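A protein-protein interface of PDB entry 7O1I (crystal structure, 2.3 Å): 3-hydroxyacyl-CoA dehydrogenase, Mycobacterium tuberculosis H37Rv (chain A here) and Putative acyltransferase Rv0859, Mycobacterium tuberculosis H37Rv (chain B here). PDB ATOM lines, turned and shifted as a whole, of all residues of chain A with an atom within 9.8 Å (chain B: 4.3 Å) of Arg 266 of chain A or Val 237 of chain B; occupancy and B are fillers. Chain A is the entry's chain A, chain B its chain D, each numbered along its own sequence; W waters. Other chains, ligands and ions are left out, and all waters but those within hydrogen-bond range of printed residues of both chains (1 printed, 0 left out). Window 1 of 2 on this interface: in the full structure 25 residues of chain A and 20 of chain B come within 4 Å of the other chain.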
ATOM      1  N   PHE A 182      -4.696  -6.199  15.087  1.00  0.00           N
ATOM      2  CA  PHE A 182      -5.631  -6.715  14.094  1.00  0.00           C
ATOM      3  C   PHE A 182      -5.497  -5.966  12.772  1.00  0.00           C
ATOM      4  O   PHE A 182      -5.257  -6.571  11.722  1.00  0.00           O
ATOM      5  CB  PHE A 182      -7.063  -6.630  14.627  1.00  0.00           C
ATOM      6  CG  PHE A 182      -8.097  -7.136  13.665  1.00  0.00           C
ATOM      7  CD1 PHE A 182      -8.250  -8.495  13.442  1.00  0.00           C
ATOM      8  CD2 PHE A 182      -8.918  -6.254  12.983  1.00  0.00           C
ATOM      9  CE1 PHE A 182      -9.201  -8.964  12.555  1.00  0.00           C
ATOM     10  CE2 PHE A 182      -9.871  -6.720  12.095  1.00  0.00           C
ATOM     11  CZ  PHE A 182     -10.014  -8.075  11.881  1.00  0.00           C
ATOM     12  N   PRO A 259     -17.551  -1.839  19.649  1.00  0.00           N
ATOM     13  CA  PRO A 259     -18.659  -2.261  18.775  1.00  0.00           C
ATOM     14  C   PRO A 259     -18.454  -1.939  17.304  1.00  0.00           C
ATOM     15  O   PRO A 259     -19.130  -2.538  16.461  1.00  0.00           O
ATOM     16  CB  PRO A 259     -19.864  -1.504  19.348  1.00  0.00           C
ATOM     17  CG  PRO A 259     -19.521  -1.288  20.765  1.00  0.00           C
ATOM     18  CD  PRO A 259     -18.046  -1.034  20.782  1.00  0.00           C
ATOM     19  N   SER A 260     -17.553  -1.018  16.964  1.00  0.00           N
ATOM     20  CA  SER A 260     -17.308  -0.695  15.565  1.00  0.00           C
ATOM     21  C   SER A 260     -16.265  -1.598  14.917  1.00  0.00           C
ATOM     22  O   SER A 260     -16.107  -1.554  13.692  1.00  0.00           O
ATOM     23  CB  SER A 260     -16.879   0.773  15.422  1.00  0.00           C
ATOM     24  OG  SER A 260     -15.562   0.984  15.903  1.00  0.00           O
ATOM     25  N   PHE A 261     -15.559  -2.422  15.701  1.00  0.00           N
ATOM     26  CA  PHE A 261     -14.542  -3.292  15.111  1.00  0.00           C
ATOM     27  C   PHE A 261     -15.149  -4.367  14.219  1.00  0.00           C
ATOM     28  O   PHE A 261     -14.630  -4.582  13.108  1.00  0.00           O
ATOM     29  CB  PHE A 261     -13.664  -3.899  16.211  1.00  0.00           C
ATOM     30  CG  PHE A 261     -12.745  -2.912  16.877  1.00  0.00           C
ATOM     31  CD1 PHE A 261     -12.729  -1.581  16.496  1.00  0.00           C
ATOM     32  CD2 PHE A 261     -11.883  -3.326  17.879  1.00  0.00           C
ATOM     33  CE1 PHE A 261     -11.882  -0.680  17.111  1.00  0.00           C
ATOM     34  CE2 PHE A 261     -11.032  -2.430  18.497  1.00  0.00           C
ATOM     35  CZ  PHE A 261     -11.032  -1.104  18.111  1.00  0.00           C
ATOM     36  N   PRO A 262     -16.210  -5.083  14.617  1.00  0.00           N
ATOM     37  CA  PRO A 262     -16.807  -6.050  13.680  1.00  0.00           C
ATOM     38  C   PRO A 262     -17.544  -5.392  12.527  1.00  0.00           C
ATOM     39  O   PRO A 262     -17.541  -5.935  11.416  1.00  0.00           O
ATOM     40  CB  PRO A 262     -17.764  -6.861  14.569  1.00  0.00           C
ATOM     41  CG  PRO A 262     -17.346  -6.578  15.965  1.00  0.00           C
ATOM     42  CD  PRO A 262     -16.833  -5.180  15.948  1.00  0.00           C
ATOM     43  N   SER A 263     -18.183  -4.241  12.757  1.00  0.00           N
ATOM     44  CA  SER A 263     -18.919  -3.582  11.682  1.00  0.00           C
ATOM     45  C   SER A 263     -17.978  -3.061  10.605  1.00  0.00           C
ATOM     46  O   SER A 263     -18.278  -3.164   9.411  1.00  0.00           O
ATOM     47  CB  SER A 263     -19.773  -2.445  12.244  1.00  0.00           C
ATOM     48  OG  SER A 263     -18.971  -1.444  12.848  1.00  0.00           O
ATOM     49  N   ASN A 264     -16.838  -2.491  11.002  1.00  0.00           N
ATOM     50  CA  ASN A 264     -15.861  -2.062  10.008  1.00  0.00           C
ATOM     51  C   ASN A 264     -15.233  -3.251   9.296  1.00  0.00           C
ATOM     52  O   ASN A 264     -14.770  -3.113   8.159  1.00  0.00           O
ATOM     53  CB  ASN A 264     -14.772  -1.205  10.652  1.00  0.00           C
ATOM     54  CG  ASN A 264     -15.205   0.236  10.866  1.00  0.00           C
ATOM     55  OD1 ASN A 264     -15.324   0.696  12.004  1.00  0.00           O
ATOM     56  ND2 ASN A 264     -15.471   0.951   9.768  1.00  0.00           N
ATOM     57  N   LEU A 265     -15.176  -4.408   9.961  1.00  0.00           N
ATOM     58  CA  LEU A 265     -14.701  -5.615   9.297  1.00  0.00           C
ATOM     59  C   LEU A 265     -15.673  -6.055   8.211  1.00  0.00           C
ATOM     60  O   LEU A 265     -15.253  -6.396   7.099  1.00  0.00           O
ATOM     61  CB  LEU A 265     -14.490  -6.732  10.317  1.00  0.00           C
ATOM     62  CG  LEU A 265     -13.914  -8.034   9.759  1.00  0.00           C
ATOM     63  CD1 LEU A 265     -12.557  -7.790   9.110  1.00  0.00           C
ATOM     64  CD2 LEU A 265     -13.807  -9.100  10.842  1.00  0.00           C
ATOM     65  N   ARG A 266     -16.976  -6.057   8.511  1.00  0.00           N
ATOM     66  CA  ARG A 266     -17.968  -6.300   7.467  1.00  0.00           C
ATOM     67  C   ARG A 266     -17.898  -5.239   6.379  1.00  0.00           C
ATOM     68  O   ARG A 266     -18.176  -5.530   5.209  1.00  0.00           O
ATOM     69  CB  ARG A 266     -19.375  -6.346   8.062  1.00  0.00           C
ATOM     70  CG  ARG A 266     -19.864  -7.744   8.394  1.00  0.00           C
ATOM     71  CD  ARG A 266     -21.345  -7.740   8.726  1.00  0.00           C
ATOM     72  NE  ARG A 266     -21.832  -9.072   9.071  1.00  0.00           N
ATOM     73  CZ  ARG A 266     -22.283  -9.954   8.186  1.00  0.00           C
ATOM     74  NH1 ARG A 266     -22.312  -9.648   6.896  1.00  0.00           N
ATOM     75  NH2 ARG A 266     -22.708 -11.145   8.590  1.00  0.00           N
ATOM     76  N   LYS A 267     -17.535  -4.006   6.743  1.00  0.00           N
ATOM     77  CA  LYS A 267     -17.366  -2.955   5.745  1.00  0.00           C
ATOM     78  C   LYS A 267     -16.259  -3.307   4.758  1.00  0.00           C
ATOM     79  O   LYS A 267     -16.412  -3.115   3.547  1.00  0.00           O
ATOM     80  CB  LYS A 267     -17.073  -1.624   6.439  1.00  0.00           C
ATOM     81  CG  LYS A 267     -16.784  -0.454   5.505  1.00  0.00           C
ATOM     82  CD  LYS A 267     -16.234   0.736   6.288  1.00  0.00           C
ATOM     83  CE  LYS A 267     -16.096   1.979   5.422  1.00  0.00           C
ATOM     84  NZ  LYS A 267     -17.418   2.585   5.100  1.00  0.00           N
ATOM     85  N   GLN A 268     -15.140  -3.835   5.257  1.00  0.00           N
ATOM     86  CA  GLN A 268     -14.035  -4.182   4.369  1.00  0.00           C
ATOM     87  C   GLN A 268     -14.332  -5.455   3.587  1.00  0.00           C
ATOM     88  O   GLN A 268     -14.100  -5.514   2.373  1.00  0.00           O
ATOM     89  CB  GLN A 268     -12.743  -4.324   5.175  1.00  0.00           C
ATOM     90  CG  GLN A 268     -12.317  -3.047   5.887  1.00  0.00           C
ATOM     91  CD  GLN A 268     -11.999  -1.918   4.922  1.00  0.00           C
ATOM     92  OE1 GLN A 268     -12.499  -0.801   5.066  1.00  0.00           O
ATOM     93  NE2 GLN A 268     -11.160  -2.205   3.933  1.00  0.00           N
ATOM     94  N   LEU A 269     -14.857  -6.480   4.259  1.00  0.00           N
ATOM     95  CA  LEU A 269     -15.173  -7.735   3.589  1.00  0.00           C
ATOM     96  C   LEU A 269     -16.425  -7.649   2.728  1.00  0.00           C
ATOM     97  O   LEU A 269     -16.672  -8.566   1.934  1.00  0.00           O
ATOM     98  CB  LEU A 269     -15.326  -8.853   4.623  1.00  0.00           C
ATOM     99  CG  LEU A 269     -14.127  -9.066   5.549  1.00  0.00           C
ATOM    100  CD1 LEU A 269     -14.351 -10.264   6.463  1.00  0.00           C
ATOM    101  CD2 LEU A 269     -12.845  -9.224   4.745  1.00  0.00           C
ATOM    102  N   LYS A 270     -17.215  -6.580   2.866  1.00  0.00           N
ATOM    103  CA  LYS A 270     -18.408  -6.355   2.045  1.00  0.00           C
ATOM    104  C   LYS A 270     -19.427  -7.478   2.202  1.00  0.00           C
ATOM    105  O   LYS A 270     -20.257  -7.705   1.319  1.00  0.00           O
ATOM    106  CB  LYS A 270     -18.039  -6.166   0.572  1.00  0.00           C
ATOM    107  CG  LYS A 270     -17.113  -4.984   0.316  1.00  0.00           C
ATOM    108  CD  LYS A 270     -16.756  -4.880  -1.155  1.00  0.00           C
ATOM    109  CE  LYS A 270     -15.820  -3.713  -1.417  1.00  0.00           C
ATOM    110  NZ  LYS A 270     -15.449  -3.608  -2.856  1.00  0.00           N
ATOM    111  N   GLY A 271     -19.376  -8.186   3.327  1.00  0.00           N
ATOM    112  CA  GLY A 271     -20.302  -9.265   3.590  1.00  0.00           C
ATOM    113  C   GLY A 271     -19.922 -10.596   2.984  1.00  0.00           C
ATOM    114  O   GLY A 271     -20.736 -11.526   3.018  1.00  0.00           O
ATOM    115  N   ALA A 272     -18.718 -10.718   2.433  1.00  0.00           N
ATOM    116  CA  ALA A 272     -18.306 -11.970   1.820  1.00  0.00           C
ATOM    117  C   ALA A 272     -18.144 -13.051   2.887  1.00  0.00           C
ATOM    118  O   ALA A 272     -17.692 -12.763   4.000  1.00  0.00           O
ATOM    119  CB  ALA A 272     -16.996 -11.788   1.053  1.00  0.00           C
ATOM    120  N   PRO A 273     -18.502 -14.304   2.582  1.00  0.00           N
ATOM    121  CA  PRO A 273     -18.423 -15.387   3.580  1.00  0.00           C
ATOM    122  C   PRO A 273     -16.994 -15.873   3.810  1.00  0.00           C
ATOM    123  O   PRO A 273     -16.657 -17.039   3.584  1.00  0.00           O
ATOM    124  CB  PRO A 273     -19.320 -16.464   2.959  1.00  0.00           C
ATOM    125  CG  PRO A 273     -19.156 -16.268   1.496  1.00  0.00           C
ATOM    126  CD  PRO A 273     -19.040 -14.779   1.295  1.00  0.00           C
ATOM    127  N   MET A 274     -16.134 -14.964   4.265  1.00  0.00           N
ATOM    128  CA  MET A 274     -14.760 -15.312   4.588  1.00  0.00           C
ATOM    129  C   MET A 274     -14.625 -15.388   6.101  1.00  0.00           C
ATOM    130  O   MET A 274     -14.688 -14.346   6.772  1.00  0.00           O
ATOM    131  CB  MET A 274     -13.793 -14.281   4.008  1.00  0.00           C
ATOM    132  CG  MET A 274     -12.353 -14.755   3.925  1.00  0.00           C
ATOM    133  SD  MET A 274     -11.441 -13.958   2.588  1.00  0.00           S
ATOM    134  CE  MET A 274     -11.753 -12.230   2.946  1.00  0.00           C
ATOM    135  N   PRO A 277     -11.037 -13.792   8.840  1.00  0.00           N
ATOM    136  CA  PRO A 277     -10.926 -12.474   9.494  1.00  0.00           C
ATOM    137  C   PRO A 277     -11.831 -12.324  10.703  1.00  0.00           C
ATOM    138  O   PRO A 277     -11.449 -11.662  11.677  1.00  0.00           O
ATOM    139  CB  PRO A 277     -11.309 -11.496   8.375  1.00  0.00           C
ATOM    140  CG  PRO A 277     -11.017 -12.231   7.117  1.00  0.00           C
ATOM    141  CD  PRO A 277     -11.374 -13.653   7.412  1.00  0.00           C
ATOM    142  N   ARG A 278     -13.025 -12.919  10.671  1.00  0.00           N
ATOM    143  CA  ARG A 278     -13.908 -12.885  11.833  1.00  0.00           C
ATOM    144  C   ARG A 278     -13.332 -13.691  12.992  1.00  0.00           C
ATOM    145  O   ARG A 278     -13.399 -13.260  14.149  1.00  0.00           O
ATOM    146  CB  ARG A 278     -15.290 -13.409  11.442  1.00  0.00           C
ATOM    147  CG  ARG A 278     -16.171 -13.814  12.606  1.00  0.00           C
ATOM    148  CD  ARG A 278     -17.360 -14.628  12.119  1.00  0.00           C
ATOM    149  NE  ARG A 278     -18.177 -15.126  13.221  1.00  0.00           N
ATOM    150  CZ  ARG A 278     -17.931 -16.254  13.880  1.00  0.00           C
ATOM    151  NH1 ARG A 278     -16.888 -17.002  13.548  1.00  0.00           N
ATOM    152  NH2 ARG A 278     -18.726 -16.634  14.871  1.00  0.00           N
ATOM    153  N   LEU A 281     -10.451 -11.754  14.705  1.00  0.00           N
ATOM    154  CA  LEU A 281     -10.953 -10.680  15.557  1.00  0.00           C
ATOM    155  C   LEU A 281     -11.603 -11.232  16.819  1.00  0.00           C
ATOM    156  O   LEU A 281     -11.421 -10.679  17.910  1.00  0.00           O
ATOM    157  CB  LEU A 281     -11.942  -9.809  14.779  1.00  0.00           C
ATOM    158  CG  LEU A 281     -12.563  -8.640  15.547  1.00  0.00           C
ATOM    159  CD1 LEU A 281     -11.474  -7.732  16.098  1.00  0.00           C
ATOM    160  CD2 LEU A 281     -13.535  -7.856  14.666  1.00  0.00           C
ATOM    161  N   GLN A 553     -25.198  -5.406  -4.247  1.00  0.00           N
ATOM    162  CA  GLN A 553     -24.933  -6.096  -2.989  1.00  0.00           C
ATOM    163  C   GLN A 553     -24.630  -7.570  -3.228  1.00  0.00           C
ATOM    164  O   GLN A 553     -23.731  -8.136  -2.597  1.00  0.00           O
ATOM    165  CB  GLN A 553     -26.117  -5.938  -2.036  1.00  0.00           C
ATOM    166  CG  GLN A 553     -26.169  -4.602  -1.314  1.00  0.00           C
ATOM    167  CD  GLN A 553     -25.091  -4.467  -0.254  1.00  0.00           C
ATOM    168  OE1 GLN A 553     -24.446  -5.447   0.125  1.00  0.00           O
ATOM    169  NE2 GLN A 553     -24.889  -3.248   0.230  1.00  0.00           N
ATOM    170  N   SER A 556     -20.930  -7.811  -4.382  1.00  0.00           N
ATOM    171  CA  SER A 556     -19.895  -7.574  -3.383  1.00  0.00           C
ATOM    172  C   SER A 556     -19.948  -8.601  -2.259  1.00  0.00           C
ATOM    173  O   SER A 556     -18.901  -8.985  -1.726  1.00  0.00           O
ATOM    174  CB  SER A 556     -20.014  -6.155  -2.833  1.00  0.00           C
ATOM    175  OG  SER A 556     -19.745  -5.206  -3.849  1.00  0.00           O
ATOM    176  N   GLN A 557     -21.144  -9.067  -1.892  1.00  0.00           N
ATOM    177  CA  GLN A 557     -21.254 -10.106  -0.875  1.00  0.00           C
ATOM    178  C   GLN A 557     -20.840 -11.476  -1.394  1.00  0.00           C
ATOM    179  O   GLN A 557     -20.538 -12.365  -0.588  1.00  0.00           O
ATOM    180  CB  GLN A 557     -22.684 -10.162  -0.329  1.00  0.00           C
ATOM    181  CG  GLN A 557     -23.099  -8.894   0.408  1.00  0.00           C
ATOM    182  CD  GLN A 557     -24.493  -8.979   0.995  1.00  0.00           C
ATOM    183  OE1 GLN A 557     -24.936 -10.044   1.427  1.00  0.00           O
ATOM    184  NE2 GLN A 557     -25.195  -7.852   1.014  1.00  0.00           N
ATOM    185  N   LEU A 648     -31.490 -13.319  -2.187  1.00  0.00           N
ATOM    186  CA  LEU A 648     -30.154 -12.796  -2.456  1.00  0.00           C
ATOM    187  C   LEU A 648     -29.153 -13.917  -2.704  1.00  0.00           C
ATOM    188  O   LEU A 648     -28.230 -13.756  -3.512  1.00  0.00           O
ATOM    189  CB  LEU A 648     -29.685 -11.919  -1.294  1.00  0.00           C
ATOM    190  CG  LEU A 648     -28.356 -11.189  -1.509  1.00  0.00           C
ATOM    191  CD1 LEU A 648     -28.520 -10.081  -2.536  1.00  0.00           C
ATOM    192  CD2 LEU A 648     -27.817 -10.640  -0.200  1.00  0.00           C
ATOM    193  N   TYR B 142     -20.606  -9.677  14.973  1.00  0.00           N
ATOM    194  CA  TYR B 142     -20.450  -9.927  13.545  1.00  0.00           C
ATOM    195  C   TYR B 142     -21.568 -10.805  12.996  1.00  0.00           C
ATOM    196  O   TYR B 142     -21.959 -10.656  11.834  1.00  0.00           O
ATOM    197  CB  TYR B 142     -19.088 -10.573  13.284  1.00  0.00           C
ATOM    198  CG  TYR B 142     -18.683 -10.677  11.829  1.00  0.00           C
ATOM    199  CD1 TYR B 142     -19.084 -11.755  11.048  1.00  0.00           C
ATOM    200  CD2 TYR B 142     -17.876  -9.709  11.245  1.00  0.00           C
ATOM    201  CE1 TYR B 142     -18.704 -11.857   9.718  1.00  0.00           C
ATOM    202  CE2 TYR B 142     -17.490  -9.804   9.916  1.00  0.00           C
ATOM    203  CZ  TYR B 142     -17.907 -10.879   9.160  1.00  0.00           C
ATOM    204  OH  TYR B 142     -17.524 -10.973   7.840  1.00  0.00           O
ATOM    205  N   MET B 145     -25.200  -9.004  13.066  1.00  0.00           N
ATOM    206  CA  MET B 145     -25.142  -7.745  12.324  1.00  0.00           C
ATOM    207  C   MET B 145     -25.717  -6.599  13.162  1.00  0.00           C
ATOM    208  O   MET B 145     -26.770  -6.029  12.873  1.00  0.00           O
ATOM    209  CB  MET B 145     -25.861  -7.873  10.974  1.00  0.00           C
ATOM    210  CG  MET B 145     -25.224  -8.880  10.024  1.00  0.00           C
ATOM    211  SD  MET B 145     -26.151  -9.093   8.491  1.00  0.00           S
ATOM    212  CE  MET B 145     -27.680  -9.782   9.120  1.00  0.00           C
ATOM    213  N   VAL B 147     -26.224  -3.054  14.549  1.00  0.00           N
ATOM    214  CA  VAL B 147     -26.112  -1.633  14.224  1.00  0.00           C
ATOM    215  C   VAL B 147     -26.843  -0.853  15.311  1.00  0.00           C
ATOM    216  O   VAL B 147     -27.819  -1.361  15.883  1.00  0.00           O
ATOM    217  CB  VAL B 147     -26.670  -1.320  12.824  1.00  0.00           C
ATOM    218  CG1 VAL B 147     -25.862  -2.035  11.747  1.00  0.00           C
ATOM    219  CG2 VAL B 147     -28.135  -1.697  12.732  1.00  0.00           C
ATOM    220  N   GLY B 233     -18.850   2.276  10.335  1.00  0.00           N
ATOM    221  CA  GLY B 233     -19.215   1.390   9.250  1.00  0.00           C
ATOM    222  C   GLY B 233     -20.558   0.717   9.413  1.00  0.00           C
ATOM    223  O   GLY B 233     -20.823  -0.284   8.744  1.00  0.00           O
ATOM    224  N   PHE B 234     -21.421   1.243  10.284  1.00  0.00           N
ATOM    225  CA  PHE B 234     -22.720   0.623  10.514  1.00  0.00           C
ATOM    226  C   PHE B 234     -23.685   0.843   9.356  1.00  0.00           C
ATOM    227  O   PHE B 234     -24.653   0.088   9.222  1.00  0.00           O
ATOM    228  CB  PHE B 234     -23.336   1.149  11.813  1.00  0.00           C
ATOM    229  CG  PHE B 234     -22.482   0.912  13.029  1.00  0.00           C
ATOM    230  CD1 PHE B 234     -22.382  -0.352  13.588  1.00  0.00           C
ATOM    231  CD2 PHE B 234     -21.786   1.955  13.618  1.00  0.00           C
ATOM    232  CE1 PHE B 234     -21.599  -0.571  14.710  1.00  0.00           C
ATOM    233  CE2 PHE B 234     -21.003   1.743  14.738  1.00  0.00           C
ATOM    234  CZ  PHE B 234     -20.909   0.477  15.284  1.00  0.00           C
ATOM    235  N   ASP B 235     -23.451   1.862   8.522  1.00  0.00           N
ATOM    236  CA  ASP B 235     -24.289   2.049   7.343  1.00  0.00           C
ATOM    237  C   ASP B 235     -24.158   0.874   6.385  1.00  0.00           C
ATOM    238  O   ASP B 235     -25.162   0.369   5.868  1.00  0.00           O
ATOM    239  CB  ASP B 235     -23.923   3.352   6.633  1.00  0.00           C
ATOM    240  CG  ASP B 235     -24.815   4.501   7.036  1.00  0.00           C
ATOM    241  OD1 ASP B 235     -25.636   4.315   7.960  1.00  0.00           O
ATOM    242  OD2 ASP B 235     -24.704   5.585   6.426  1.00  0.00           O
ATOM    243  N   ASP B 236     -22.927   0.420   6.140  1.00  0.00           N
ATOM    244  CA  ASP B 236     -22.715  -0.686   5.213  1.00  0.00           C
ATOM    245  C   ASP B 236     -23.273  -1.990   5.768  1.00  0.00           C
ATOM    246  O   ASP B 236     -23.787  -2.821   5.010  1.00  0.00           O
ATOM    247  CB  ASP B 236     -21.225  -0.822   4.901  1.00  0.00           C
ATOM    248  CG  ASP B 236     -20.622   0.460   4.360  1.00  0.00           C
ATOM    249  OD1 ASP B 236     -21.216   1.058   3.436  1.00  0.00           O
ATOM    250  OD2 ASP B 236     -19.561   0.880   4.865  1.00  0.00           O
ATOM    251  N   VAL B 237     -23.185  -2.187   7.086  1.00  0.00           N
ATOM    252  CA  VAL B 237     -23.725  -3.401   7.691  1.00  0.00           C
ATOM    253  C   VAL B 237     -25.238  -3.457   7.516  1.00  0.00           C
ATOM    254  O   VAL B 237     -25.802  -4.507   7.184  1.00  0.00           O
ATOM    255  CB  VAL B 237     -23.323  -3.483   9.175  1.00  0.00           C
ATOM    256  CG1 VAL B 237     -23.996  -4.670   9.846  1.00  0.00           C
ATOM    257  CG2 VAL B 237     -21.811  -3.579   9.307  1.00  0.00           C
ATOM    258  N   ALA B 238     -25.918  -2.328   7.726  1.00  0.00           N
ATOM    259  CA  ALA B 238     -27.370  -2.298   7.580  1.00  0.00           C
ATOM    260  C   ALA B 238     -27.804  -2.528   6.137  1.00  0.00           C
ATOM    261  O   ALA B 238     -28.866  -3.113   5.899  1.00  0.00           O
ATOM    262  CB  ALA B 238     -27.922  -0.969   8.094  1.00  0.00           C
ATOM    263  N   LEU B 239     -27.004  -2.084   5.166  1.00  0.00           N
ATOM    264  CA  LEU B 239     -27.358  -2.257   3.761  1.00  0.00           C
ATOM    265  C   LEU B 239     -27.007  -3.638   3.224  1.00  0.00           C
ATOM    266  O   LEU B 239     -27.402  -3.965   2.100  1.00  0.00           O
ATOM    267  CB  LEU B 239     -26.681  -1.182   2.906  1.00  0.00           C
ATOM    268  CG  LEU B 239     -27.067   0.263   3.233  1.00  0.00           C
ATOM    269  CD1 LEU B 239     -26.438   1.234   2.243  1.00  0.00           C
ATOM    270  CD2 LEU B 239     -28.580   0.420   3.271  1.00  0.00           C
ATOM    271  N   GLN B 240     -26.273  -4.453   3.985  1.00  0.00           N
ATOM    272  CA  GLN B 240     -26.064  -5.836   3.573  1.00  0.00           C
ATOM    273  C   GLN B 240     -27.297  -6.683   3.858  1.00  0.00           C
ATOM    274  O   GLN B 240     -27.648  -7.564   3.064  1.00  0.00           O
ATOM    275  CB  GLN B 240     -24.833  -6.414   4.273  1.00  0.00           C
ATOM    276  CG  GLN B 240     -23.523  -5.773   3.843  1.00  0.00           C
ATOM    277  CD  GLN B 240     -22.333  -6.287   4.632  1.00  0.00           C
ATOM    278  OE1 GLN B 240     -22.471  -7.163   5.487  1.00  0.00           O
ATOM    279  NE2 GLN B 240     -21.156  -5.741   4.349  1.00  0.00           N
ATOM    280  N   LYS B 241     -27.966  -6.424   4.985  1.00  0.00           N
ATOM    281  CA  LYS B 241     -29.238  -7.078   5.273  1.00  0.00           C
ATOM    282  C   LYS B 241     -30.345  -6.528   4.381  1.00  0.00           C
ATOM    283  O   LYS B 241     -31.127  -7.290   3.797  1.00  0.00           O
ATOM    284  CB  LYS B 241     -29.588  -6.894   6.751  1.00  0.00           C
ATOM    285  CG  LYS B 241     -30.964  -7.400   7.155  1.00  0.00           C
ATOM    286  CD  LYS B 241     -30.972  -8.905   7.358  1.00  0.00           C
ATOM    287  CE  LYS B 241     -32.312  -9.373   7.905  1.00  0.00           C
ATOM    288  NZ  LYS B 241     -32.323 -10.833   8.203  1.00  0.00           N
HETATM  289  O   HOH W   1     -20.193   3.253   6.747  1.00  0.00           O
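O of Tyr 142 of chain B sits at hydrogen-bond distance from NE of Arg 266 of chain A (3.2 Å). OD2 of Asp 236 of chain B is in salt-bridge range of NZ of Lys 267 of chain A (2.7 Å). O of Leu 239 of chain B lies within hydrogen-bond range of NE2 of Gln 553 of chain A (3.2 Å). OE1 of Gln 240 of chain B lies within hydrogen-bond range of NH1 of Arg 266 of chain A (2.9 Å). NE2 of Gln 240 of chain B sits close to N of Gly 271 of chain A (3.2 Å). The backbone carbonyl oxygen (O) of Gln 240 of chain B sits at hydrogen-bond distance from the side-chain amide nitrogen (NE2) of Gln 557 of chain A, at 3.2 Å.
O of Ser 260 of chain A is in hydrogen-bond range of OG of Ser 263 of chain A (3.0 Å). O of Ser 260 of chain A sits close to OD1 of Asn 264 of chain A, 2.9 Å away. N of Gly 271 of chain A sits at hydrogen-bond distance from O of Arg 266 of chain A (3.5 Å). OE1 of Gln 553 of chain A lies within hydrogen-bond range of NE2 of Gln 557 of chain A (2.7 Å).
Pro 259 of chain A touches Phe 234 of chain B (O to CE1, 3.6 Å). Phe 234 of chain B touches Ser 260 of chain A (CZ to CA, 3.8 Å). CD2 of Tyr 142 of chain B touches O of Pro 262 of chain A (3.8 Å). Ser 263 of chain A touches Gly 233 of chain B (O to O, 3.9 Å). Ser 263 of chain A touches Phe 234 of chain B (OG to CE1, 3.3 Å). Asn 264 of chain A touches Gly 233 of chain B (ND2 to N, 3.7 Å). Met 145 of chain B touches Arg 266 of chain A (CG to NE, 3.5 Å). Tyr 142 of chain B touches Leu 269 of chain A (OH to CD1, 3.5 Å). Lys 270 of chain A touches Gln 240 of chain B (C to NE2, 3.3 Å). OE1 of Gln 553 of chain A touches CA of Gln 240 of chain B, at 3.8 Å.
Printed residues of chain B within 4 Å of Arg 266 of chain A: Tyr 142, Met 145, Val 237 and Gln 240. Val 237 of chain B touches just these residues of chain A: Ser 263 (3.6 Å) and Arg 266 (3.9 Å). Of chain A, only Arg 266 (3.5 Å) comes within 4 Å of Met 145 of chain B. No residue of chain A comes within 4 Å of Ala 238 of chain B. Printed residues of chain B within 4 Å of Gly 271 of chain A: Gln 240 (3.2 Å). Of the printed residues of chain B, Asn 264 of chain A touches Gly 233. Of the printed residues of chain A, Gly 233 of chain B touches Ser 263 and Asn 264. Asp 235 of chain B touches none of the printed residues of chain A. The nearest printed residue of chain B that does not touch Arg 266 of chain A is Asp 236 of chain B (5.6 Å). The nearest residue of chain A that does not touch Val 237 of chain B is Lys 267 of chain A (5.0 Å). The nearest printed residue of chain A that does not touch Phe 234 of chain B is Asn 264 of chain A (6.0 Å).
Printed residues of chain A that touch a printed residue of chain B: Pro 259, Ser 260, Pro 262, Ser 263, Asn 264, Leu 265, Arg 266, Lys 267, Leu 269, Lys 270, Gly 271, Arg 278, Gln 553 and Gln 557. Hydrophobic or aromatic side chains of chain A that line the printed part of chain B: Leu 265 and Leu 269. Hydrophobic or aromatic side chains of chain B within 4 Å of the printed part of chain A: Tyr 142, Met 145, Phe 234, Val 237 and Leu 239. Among the printed residues, Asp or Glu carboxylates within 4 Å of a Lys or Arg side-chain nitrogen of the other chain: Lys 267 of chain A with Asp 236 of chain B.
Water W1 lies within hydrogen-bond range of the side-chain carboxylate (OD2) of Asp 236 of chain B (3.1 Å) and the side-chain amino group (NZ) of Lys 267 of chain A (3.3 Å).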
